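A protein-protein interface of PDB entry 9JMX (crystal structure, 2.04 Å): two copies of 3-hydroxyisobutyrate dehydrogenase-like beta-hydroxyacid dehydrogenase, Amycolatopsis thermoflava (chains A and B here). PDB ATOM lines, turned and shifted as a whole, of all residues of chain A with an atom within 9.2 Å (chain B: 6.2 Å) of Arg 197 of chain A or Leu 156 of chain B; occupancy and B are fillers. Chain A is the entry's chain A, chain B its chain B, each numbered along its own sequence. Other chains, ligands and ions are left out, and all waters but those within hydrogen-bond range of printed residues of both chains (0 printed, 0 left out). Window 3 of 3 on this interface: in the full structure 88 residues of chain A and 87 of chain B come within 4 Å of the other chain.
N of Tyr 133 of chain B lies within hydrogen-bond range of O of Glu 154 of chain B, 2.7 Å away.
N of Leu 156 of chain B sits at hydrogen-bond distance from O of Tyr 133 of chain B, at 2.7 Å.
Leu 156 of chain B touches Arg 197 of chain A (CD2 to NH2, 3.2 Å).
CD1 of Leu 198 of chain A touches CD2 of Phe 166 of chain B (3.7 Å).
Phe 201 of chain A touches Phe 132 of chain B.
Phe 201 of chain A touches Glu 154 of chain B.
Of chain B, only Leu 156 comes within 4 Å of Arg 197 of chain A.
Leu 156 of chain B touches just one residue of chain A: Arg 197 (3.2 Å).
No residue of chain A comes within 4 Å of Gly 157 of chain B.
No residue of chain A comes within 4 Å of Ala 163 of chain B.
Printed residues of chain A within 4 Å of Phe 166 of chain B: Leu 198.
Of the printed residues of chain B, Phe 201 of chain A touches Phe 132 (3.7 Å) and Glu 154 (3.7 Å).
The nearest residue of chain B that does not touch Arg 197 of chain A is Phe 166 of chain B (4.02 Å).
The nearest residue of chain A that does not touch Leu 156 of chain B is Phe 201 of chain A (5.5 Å).
Of the 14 printed residues of chain A, 3 touch a printed residue of chain B.
Hydrophobic or aromatic side chains of chain A within 4 Å of the printed part of chain B: Leu 198 and Phe 201.
Along chain A the printed residues that touch a printed residue of chain B span positions 197 to 201.
Among the printed residues, no Asp or Glu carboxylate lies within 4 Å of a Lys or Arg side-chain nitrogen of the other chain.
No position is printed for both chains.
Of the 4 pairs that touch across the chains among the printed residues, none has its exchanged pair printed and touching as well.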
ATOM      1  N   PHE A 185      32.706 -35.215  -7.167  1.00  0.00           N
ATOM      2  CA  PHE A 185      31.854 -36.320  -7.649  1.00  0.00           C
ATOM      3  C   PHE A 185      31.391 -37.176  -6.457  1.00  0.00           C
ATOM      4  O   PHE A 185      30.246 -37.638  -6.469  1.00  0.00           O
ATOM      5  CB  PHE A 185      32.584 -37.162  -8.690  1.00  0.00           C
ATOM      6  CG  PHE A 185      32.812 -36.514 -10.028  1.00  0.00           C
ATOM      7  CD1 PHE A 185      32.098 -35.401 -10.430  1.00  0.00           C
ATOM      8  CD2 PHE A 185      33.707 -37.075 -10.918  1.00  0.00           C
ATOM      9  CE1 PHE A 185      32.306 -34.835 -11.681  1.00  0.00           C
ATOM     10  CE2 PHE A 185      33.946 -36.481 -12.149  1.00  0.00           C
ATOM     11  CZ  PHE A 185      33.241 -35.363 -12.527  1.00  0.00           C
ATOM     12  N   LEU A 188      28.489 -35.504  -4.557  1.00  0.00           N
ATOM     13  CA  LEU A 188      27.211 -35.682  -5.305  1.00  0.00           C
ATOM     14  C   LEU A 188      26.732 -37.130  -5.134  1.00  0.00           C
ATOM     15  O   LEU A 188      25.562 -37.333  -4.737  1.00  0.00           O
ATOM     16  CB  LEU A 188      27.385 -35.397  -6.795  1.00  0.00           C
ATOM     17  CG  LEU A 188      27.620 -33.947  -7.237  1.00  0.00           C
ATOM     18  CD1 LEU A 188      27.133 -33.757  -8.675  1.00  0.00           C
ATOM     19  CD2 LEU A 188      26.933 -32.938  -6.353  1.00  0.00           C
ATOM     20  N   GLY A 192      23.124 -38.907  -3.548  1.00  0.00           N
ATOM     21  CA  GLY A 192      22.195 -39.514  -4.504  1.00  0.00           C
ATOM     22  C   GLY A 192      22.109 -38.772  -5.823  1.00  0.00           C
ATOM     23  O   GLY A 192      21.310 -39.208  -6.660  1.00  0.00           O
ATOM     24  N   ALA A 193      22.906 -37.727  -6.053  1.00  0.00           N
ATOM     25  CA  ALA A 193      22.921 -36.989  -7.332  1.00  0.00           C
ATOM     26  C   ALA A 193      23.941 -37.640  -8.269  1.00  0.00           C
ATOM     27  O   ALA A 193      24.780 -38.401  -7.802  1.00  0.00           O
ATOM     28  CB  ALA A 193      23.213 -35.531  -7.100  1.00  0.00           C
ATOM     29  N   ASP A 194      23.851 -37.335  -9.562  1.00  0.00           N
ATOM     30  CA  ASP A 194      24.626 -37.968 -10.648  1.00  0.00           C
ATOM     31  C   ASP A 194      25.856 -37.108 -10.949  1.00  0.00           C
ATOM     32  O   ASP A 194      25.722 -36.009 -11.482  1.00  0.00           O
ATOM     33  CB  ASP A 194      23.747 -38.137 -11.885  1.00  0.00           C
ATOM     34  CG  ASP A 194      24.456 -38.858 -13.001  1.00  0.00           C
ATOM     35  OD1 ASP A 194      25.602 -39.260 -12.763  1.00  0.00           O
ATOM     36  OD2 ASP A 194      23.853 -39.008 -14.101  1.00  0.00           O
ATOM     37  N   PRO A 195      27.084 -37.591 -10.637  1.00  0.00           N
ATOM     38  CA  PRO A 195      28.316 -36.879 -10.977  1.00  0.00           C
ATOM     39  C   PRO A 195      28.321 -36.376 -12.424  1.00  0.00           C
ATOM     40  O   PRO A 195      28.804 -35.293 -12.631  1.00  0.00           O
ATOM     41  CB  PRO A 195      29.422 -37.931 -10.784  1.00  0.00           C
ATOM     42  CG  PRO A 195      28.863 -38.832  -9.720  1.00  0.00           C
ATOM     43  CD  PRO A 195      27.374 -38.887 -10.012  1.00  0.00           C
ATOM     44  N   ALA A 196      27.785 -37.165 -13.371  1.00  0.00           N
ATOM     45  CA  ALA A 196      27.664 -36.791 -14.802  1.00  0.00           C
ATOM     46  C   ALA A 196      27.072 -35.384 -14.937  1.00  0.00           C
ATOM     47  O   ALA A 196      27.492 -34.681 -15.853  1.00  0.00           O
ATOM     48  CB  ALA A 196      26.810 -37.786 -15.548  1.00  0.00           C
ATOM     49  N   ARG A 197      26.114 -35.003 -14.090  1.00  0.00           N
ATOM     50  CA  ARG A 197      25.402 -33.703 -14.209  1.00  0.00           C
ATOM     51  C   ARG A 197      26.337 -32.556 -13.822  1.00  0.00           C
ATOM     52  O   ARG A 197      26.015 -31.404 -14.158  1.00  0.00           O
ATOM     53  CB  ARG A 197      24.172 -33.611 -13.300  1.00  0.00           C
ATOM     54  CG  ARG A 197      23.007 -34.509 -13.696  1.00  0.00           C
ATOM     55  CD  ARG A 197      21.813 -34.308 -12.766  1.00  0.00           C
ATOM     56  NE  ARG A 197      21.240 -32.958 -12.821  1.00  0.00           N
ATOM     57  CZ  ARG A 197      20.237 -32.519 -12.054  1.00  0.00           C
ATOM     58  NH1 ARG A 197      19.684 -33.310 -11.149  1.00  0.00           N
ATOM     59  NH2 ARG A 197      19.784 -31.286 -12.195  1.00  0.00           N
ATOM     60  N   LEU A 198      27.414 -32.827 -13.081  1.00  0.00           N
ATOM     61  CA  LEU A 198      28.317 -31.744 -12.651  1.00  0.00           C
ATOM     62  C   LEU A 198      29.256 -31.360 -13.796  1.00  0.00           C
ATOM     63  O   LEU A 198      29.778 -30.220 -13.767  1.00  0.00           O
ATOM     64  CB  LEU A 198      29.100 -32.139 -11.398  1.00  0.00           C
ATOM     65  CG  LEU A 198      29.730 -30.948 -10.674  1.00  0.00           C
ATOM     66  CD1 LEU A 198      28.657 -30.060 -10.058  1.00  0.00           C
ATOM     67  CD2 LEU A 198      30.753 -31.399  -9.627  1.00  0.00           C
ATOM     68  N   VAL A 199      29.489 -32.260 -14.743  1.00  0.00           N
ATOM     69  CA  VAL A 199      30.659 -32.170 -15.668  1.00  0.00           C
ATOM     70  C   VAL A 199      30.719 -30.781 -16.309  1.00  0.00           C
ATOM     71  O   VAL A 199      31.712 -30.063 -16.147  1.00  0.00           O
ATOM     72  CB  VAL A 199      30.664 -33.315 -16.701  1.00  0.00           C
ATOM     73  CG1 VAL A 199      31.650 -33.072 -17.845  1.00  0.00           C
ATOM     74  CG2 VAL A 199      30.978 -34.628 -15.999  1.00  0.00           C
ATOM     75  N   PRO A 200      29.672 -30.336 -17.043  1.00  0.00           N
ATOM     76  CA  PRO A 200      29.733 -29.045 -17.715  1.00  0.00           C
ATOM     77  C   PRO A 200      30.072 -27.921 -16.733  1.00  0.00           C
ATOM     78  O   PRO A 200      30.851 -27.079 -17.085  1.00  0.00           O
ATOM     79  CB  PRO A 200      28.349 -28.842 -18.338  1.00  0.00           C
ATOM     80  CG  PRO A 200      27.481 -29.935 -17.737  1.00  0.00           C
ATOM     81  CD  PRO A 200      28.412 -31.044 -17.316  1.00  0.00           C
ATOM     82  N   PHE A 201      29.519 -27.941 -15.529  1.00  0.00           N
ATOM     83  CA  PHE A 201      29.761 -26.886 -14.513  1.00  0.00           C
ATOM     84  C   PHE A 201      31.192 -27.001 -13.956  1.00  0.00           C
ATOM     85  O   PHE A 201      31.741 -25.975 -13.511  1.00  0.00           O
ATOM     86  CB  PHE A 201      28.713 -26.952 -13.397  1.00  0.00           C
ATOM     87  CG  PHE A 201      27.296 -27.058 -13.908  1.00  0.00           C
ATOM     88  CD1 PHE A 201      26.690 -25.984 -14.544  1.00  0.00           C
ATOM     89  CD2 PHE A 201      26.575 -28.245 -13.794  1.00  0.00           C
ATOM     90  CE1 PHE A 201      25.385 -26.081 -15.016  1.00  0.00           C
ATOM     91  CE2 PHE A 201      25.274 -28.344 -14.289  1.00  0.00           C
ATOM     92  CZ  PHE A 201      24.686 -27.262 -14.907  1.00  0.00           C
ATOM     93  N   ALA A 202      31.753 -28.212 -13.911  1.00  0.00           N
ATOM     94  CA  ALA A 202      33.125 -28.457 -13.415  1.00  0.00           C
ATOM     95  C   ALA A 202      34.100 -27.822 -14.411  1.00  0.00           C
ATOM     96  O   ALA A 202      35.083 -27.184 -13.962  1.00  0.00           O
ATOM     97  CB  ALA A 202      33.374 -29.934 -13.222  1.00  0.00           C
ATOM     98  N   ARG A 203      33.820 -27.971 -15.707  1.00  0.00           N
ATOM     99  CA  ARG A 203      34.654 -27.367 -16.783  1.00  0.00           C
ATOM    100  C   ARG A 203      34.633 -25.856 -16.608  1.00  0.00           C
ATOM    101  O   ARG A 203      35.724 -25.199 -16.696  1.00  0.00           O
ATOM    102  CB  ARG A 203      34.114 -27.645 -18.180  1.00  0.00           C
ATOM    103  CG  ARG A 203      34.403 -29.029 -18.730  1.00  0.00           C
ATOM    104  CD  ARG A 203      33.940 -29.106 -20.184  1.00  0.00           C
ATOM    105  NE  ARG A 203      33.408 -30.426 -20.458  1.00  0.00           N
ATOM    106  CZ  ARG A 203      34.145 -31.521 -20.534  1.00  0.00           C
ATOM    107  NH1 ARG A 203      35.465 -31.475 -20.365  1.00  0.00           N
ATOM    108  NH2 ARG A 203      33.553 -32.672 -20.769  1.00  0.00           N
ATOM    109  N   PHE B 132      22.727 -21.901  -9.642  1.00  0.00           N
ATOM    110  CA  PHE B 132      21.977 -23.133  -9.303  1.00  0.00           C
ATOM    111  C   PHE B 132      20.781 -22.706  -8.447  1.00  0.00           C
ATOM    112  O   PHE B 132      20.941 -21.800  -7.606  1.00  0.00           O
ATOM    113  CB  PHE B 132      22.845 -24.121  -8.536  1.00  0.00           C
ATOM    114  CG  PHE B 132      24.045 -24.632  -9.283  1.00  0.00           C
ATOM    115  CD1 PHE B 132      23.904 -25.321 -10.479  1.00  0.00           C
ATOM    116  CD2 PHE B 132      25.307 -24.507  -8.731  1.00  0.00           C
ATOM    117  CE1 PHE B 132      25.003 -25.854 -11.133  1.00  0.00           C
ATOM    118  CE2 PHE B 132      26.403 -25.050  -9.385  1.00  0.00           C
ATOM    119  CZ  PHE B 132      26.262 -25.667 -10.605  1.00  0.00           C
ATOM    120  N   TYR B 133      19.620 -23.315  -8.666  1.00  0.00           N
ATOM    121  CA  TYR B 133      18.418 -23.108  -7.811  1.00  0.00           C
ATOM    122  C   TYR B 133      17.748 -24.446  -7.530  1.00  0.00           C
ATOM    123  O   TYR B 133      17.743 -25.373  -8.374  1.00  0.00           O
ATOM    124  CB  TYR B 133      17.379 -22.201  -8.473  1.00  0.00           C
ATOM    125  CG  TYR B 133      17.806 -20.770  -8.646  1.00  0.00           C
ATOM    126  CD1 TYR B 133      17.775 -19.865  -7.598  1.00  0.00           C
ATOM    127  CD2 TYR B 133      18.243 -20.331  -9.879  1.00  0.00           C
ATOM    128  CE1 TYR B 133      18.153 -18.540  -7.774  1.00  0.00           C
ATOM    129  CE2 TYR B 133      18.623 -19.017 -10.072  1.00  0.00           C
ATOM    130  CZ  TYR B 133      18.590 -18.118  -9.024  1.00  0.00           C
ATOM    131  OH  TYR B 133      19.001 -16.836  -9.284  1.00  0.00           O
ATOM    132  N   SER B 134      17.171 -24.531  -6.344  1.00  0.00           N
ATOM    133  CA  SER B 134      16.426 -25.724  -5.887  1.00  0.00           C
ATOM    134  C   SER B 134      15.433 -25.241  -4.835  1.00  0.00           C
ATOM    135  O   SER B 134      15.728 -24.264  -4.129  1.00  0.00           O
ATOM    136  CB  SER B 134      17.372 -26.793  -5.358  1.00  0.00           C
ATOM    137  OG  SER B 134      18.052 -26.327  -4.192  1.00  0.00           O
ATOM    138  N   GLU B 154      19.790 -22.250 -13.319  1.00  0.00           N
ATOM    139  CA  GLU B 154      19.850 -23.726 -13.436  1.00  0.00           C
ATOM    140  C   GLU B 154      19.016 -24.304 -12.299  1.00  0.00           C
ATOM    141  O   GLU B 154      19.558 -24.429 -11.156  1.00  0.00           O
ATOM    142  CB  GLU B 154      21.309 -24.196 -13.392  1.00  0.00           C
ATOM    143  CG  GLU B 154      21.492 -25.680 -13.605  1.00  0.00           C
ATOM    144  CD  GLU B 154      21.180 -26.235 -14.980  1.00  0.00           C
ATOM    145  OE1 GLU B 154      21.463 -25.551 -15.979  1.00  0.00           O
ATOM    146  OE2 GLU B 154      20.720 -27.401 -15.053  1.00  0.00           O
ATOM    147  N   TYR B 155      17.747 -24.606 -12.582  1.00  0.00           N
ATOM    148  CA  TYR B 155      16.806 -25.215 -11.602  1.00  0.00           C
ATOM    149  C   TYR B 155      17.070 -26.724 -11.544  1.00  0.00           C
ATOM    150  O   TYR B 155      16.891 -27.410 -12.555  1.00  0.00           O
ATOM    151  CB  TYR B 155      15.328 -24.927 -11.906  1.00  0.00           C
ATOM    152  CG  TYR B 155      14.401 -25.547 -10.887  1.00  0.00           C
ATOM    153  CD1 TYR B 155      14.183 -24.932  -9.662  1.00  0.00           C
ATOM    154  CD2 TYR B 155      13.774 -26.763 -11.122  1.00  0.00           C
ATOM    155  CE1 TYR B 155      13.361 -25.510  -8.705  1.00  0.00           C
ATOM    156  CE2 TYR B 155      12.923 -27.334 -10.188  1.00  0.00           C
ATOM    157  CZ  TYR B 155      12.731 -26.719  -8.967  1.00  0.00           C
ATOM    158  OH  TYR B 155      11.932 -27.293  -8.013  1.00  0.00           O
ATOM    159  N   LEU B 156      17.434 -27.226 -10.365  1.00  0.00           N
ATOM    160  CA  LEU B 156      17.918 -28.615 -10.182  1.00  0.00           C
ATOM    161  C   LEU B 156      16.787 -29.539  -9.697  1.00  0.00           C
ATOM    162  O   LEU B 156      16.890 -30.756  -9.978  1.00  0.00           O
ATOM    163  CB  LEU B 156      19.105 -28.595  -9.209  1.00  0.00           C
ATOM    164  CG  LEU B 156      20.351 -27.871  -9.718  1.00  0.00           C
ATOM    165  CD1 LEU B 156      21.382 -27.679  -8.611  1.00  0.00           C
ATOM    166  CD2 LEU B 156      20.956 -28.619 -10.883  1.00  0.00           C
ATOM    167  N   GLY B 157      15.771 -29.012  -8.999  1.00  0.00           N
ATOM    168  CA  GLY B 157      14.648 -29.827  -8.489  1.00  0.00           C
ATOM    169  C   GLY B 157      14.150 -29.353  -7.141  1.00  0.00           C
ATOM    170  O   GLY B 157      14.517 -28.235  -6.709  1.00  0.00           O
ATOM    171  N   GLU B 158      13.336 -30.179  -6.486  1.00  0.00           N
ATOM    172  CA  GLU B 158      12.467 -29.750  -5.355  1.00  0.00           C
ATOM    173  C   GLU B 158      13.309 -29.689  -4.078  1.00  0.00           C
ATOM    174  O   GLU B 158      13.101 -28.782  -3.243  1.00  0.00           O
ATOM    175  CB  GLU B 158      11.253 -30.680  -5.273  1.00  0.00           C
ATOM    176  CG  GLU B 158      10.215 -30.396  -6.361  1.00  0.00           C
ATOM    177  CD  GLU B 158       9.456 -29.093  -6.165  1.00  0.00           C
ATOM    178  OE1 GLU B 158       8.974 -28.515  -7.167  1.00  0.00           O
ATOM    179  OE2 GLU B 158       9.371 -28.648  -5.011  1.00  0.00           O
ATOM    180  N   LEU B 162      19.777 -29.301  -3.017  1.00  0.00           N
ATOM    181  CA  LEU B 162      20.404 -29.647  -4.315  1.00  0.00           C
ATOM    182  C   LEU B 162      21.328 -28.513  -4.776  1.00  0.00           C
ATOM    183  O   LEU B 162      22.463 -28.817  -5.155  1.00  0.00           O
ATOM    184  CB  LEU B 162      19.321 -29.943  -5.352  1.00  0.00           C
ATOM    185  CG  LEU B 162      18.988 -31.419  -5.529  1.00  0.00           C
ATOM    186  CD1 LEU B 162      17.660 -31.582  -6.254  1.00  0.00           C
ATOM    187  CD2 LEU B 162      20.104 -32.151  -6.264  1.00  0.00           C
ATOM    188  N   ALA B 163      20.862 -27.267  -4.768  1.00  0.00           N
ATOM    189  CA  ALA B 163      21.650 -26.105  -5.243  1.00  0.00           C
ATOM    190  C   ALA B 163      22.882 -25.982  -4.345  1.00  0.00           C
ATOM    191  O   ALA B 163      23.961 -25.698  -4.856  1.00  0.00           O
ATOM    192  CB  ALA B 163      20.845 -24.827  -5.221  1.00  0.00           C
ATOM    193  N   GLN B 164      22.705 -26.181  -3.039  1.00  0.00           N
ATOM    194  CA  GLN B 164      23.802 -26.077  -2.052  1.00  0.00           C
ATOM    195  C   GLN B 164      24.814 -27.204  -2.327  1.00  0.00           C
ATOM    196  O   GLN B 164      26.036 -26.925  -2.309  1.00  0.00           O
ATOM    197  CB  GLN B 164      23.221 -26.082  -0.642  1.00  0.00           C
ATOM    198  CG  GLN B 164      24.212 -25.657   0.421  1.00  0.00           C
ATOM    199  CD  GLN B 164      24.626 -24.205   0.323  1.00  0.00           C
ATOM    200  OE1 GLN B 164      25.629 -23.876  -0.327  1.00  0.00           O
ATOM    201  NE2 GLN B 164      23.917 -23.335   1.041  1.00  0.00           N
ATOM    202  N   PHE B 166      25.395 -28.808  -5.279  1.00  0.00           N
ATOM    203  CA  PHE B 166      26.121 -28.511  -6.550  1.00  0.00           C
ATOM    204  C   PHE B 166      27.069 -27.345  -6.289  1.00  0.00           C
ATOM    205  O   PHE B 166      28.196 -27.418  -6.749  1.00  0.00           O
ATOM    206  CB  PHE B 166      25.159 -28.251  -7.707  1.00  0.00           C
ATOM    207  CG  PHE B 166      24.691 -29.497  -8.408  1.00  0.00           C
ATOM    208  CD1 PHE B 166      23.948 -30.451  -7.740  1.00  0.00           C
ATOM    209  CD2 PHE B 166      24.954 -29.696  -9.751  1.00  0.00           C
ATOM    210  CE1 PHE B 166      23.521 -31.592  -8.394  1.00  0.00           C
ATOM    211  CE2 PHE B 166      24.515 -30.836 -10.405  1.00  0.00           C
ATOM    212  CZ  PHE B 166      23.803 -31.783  -9.719  1.00  0.00           C
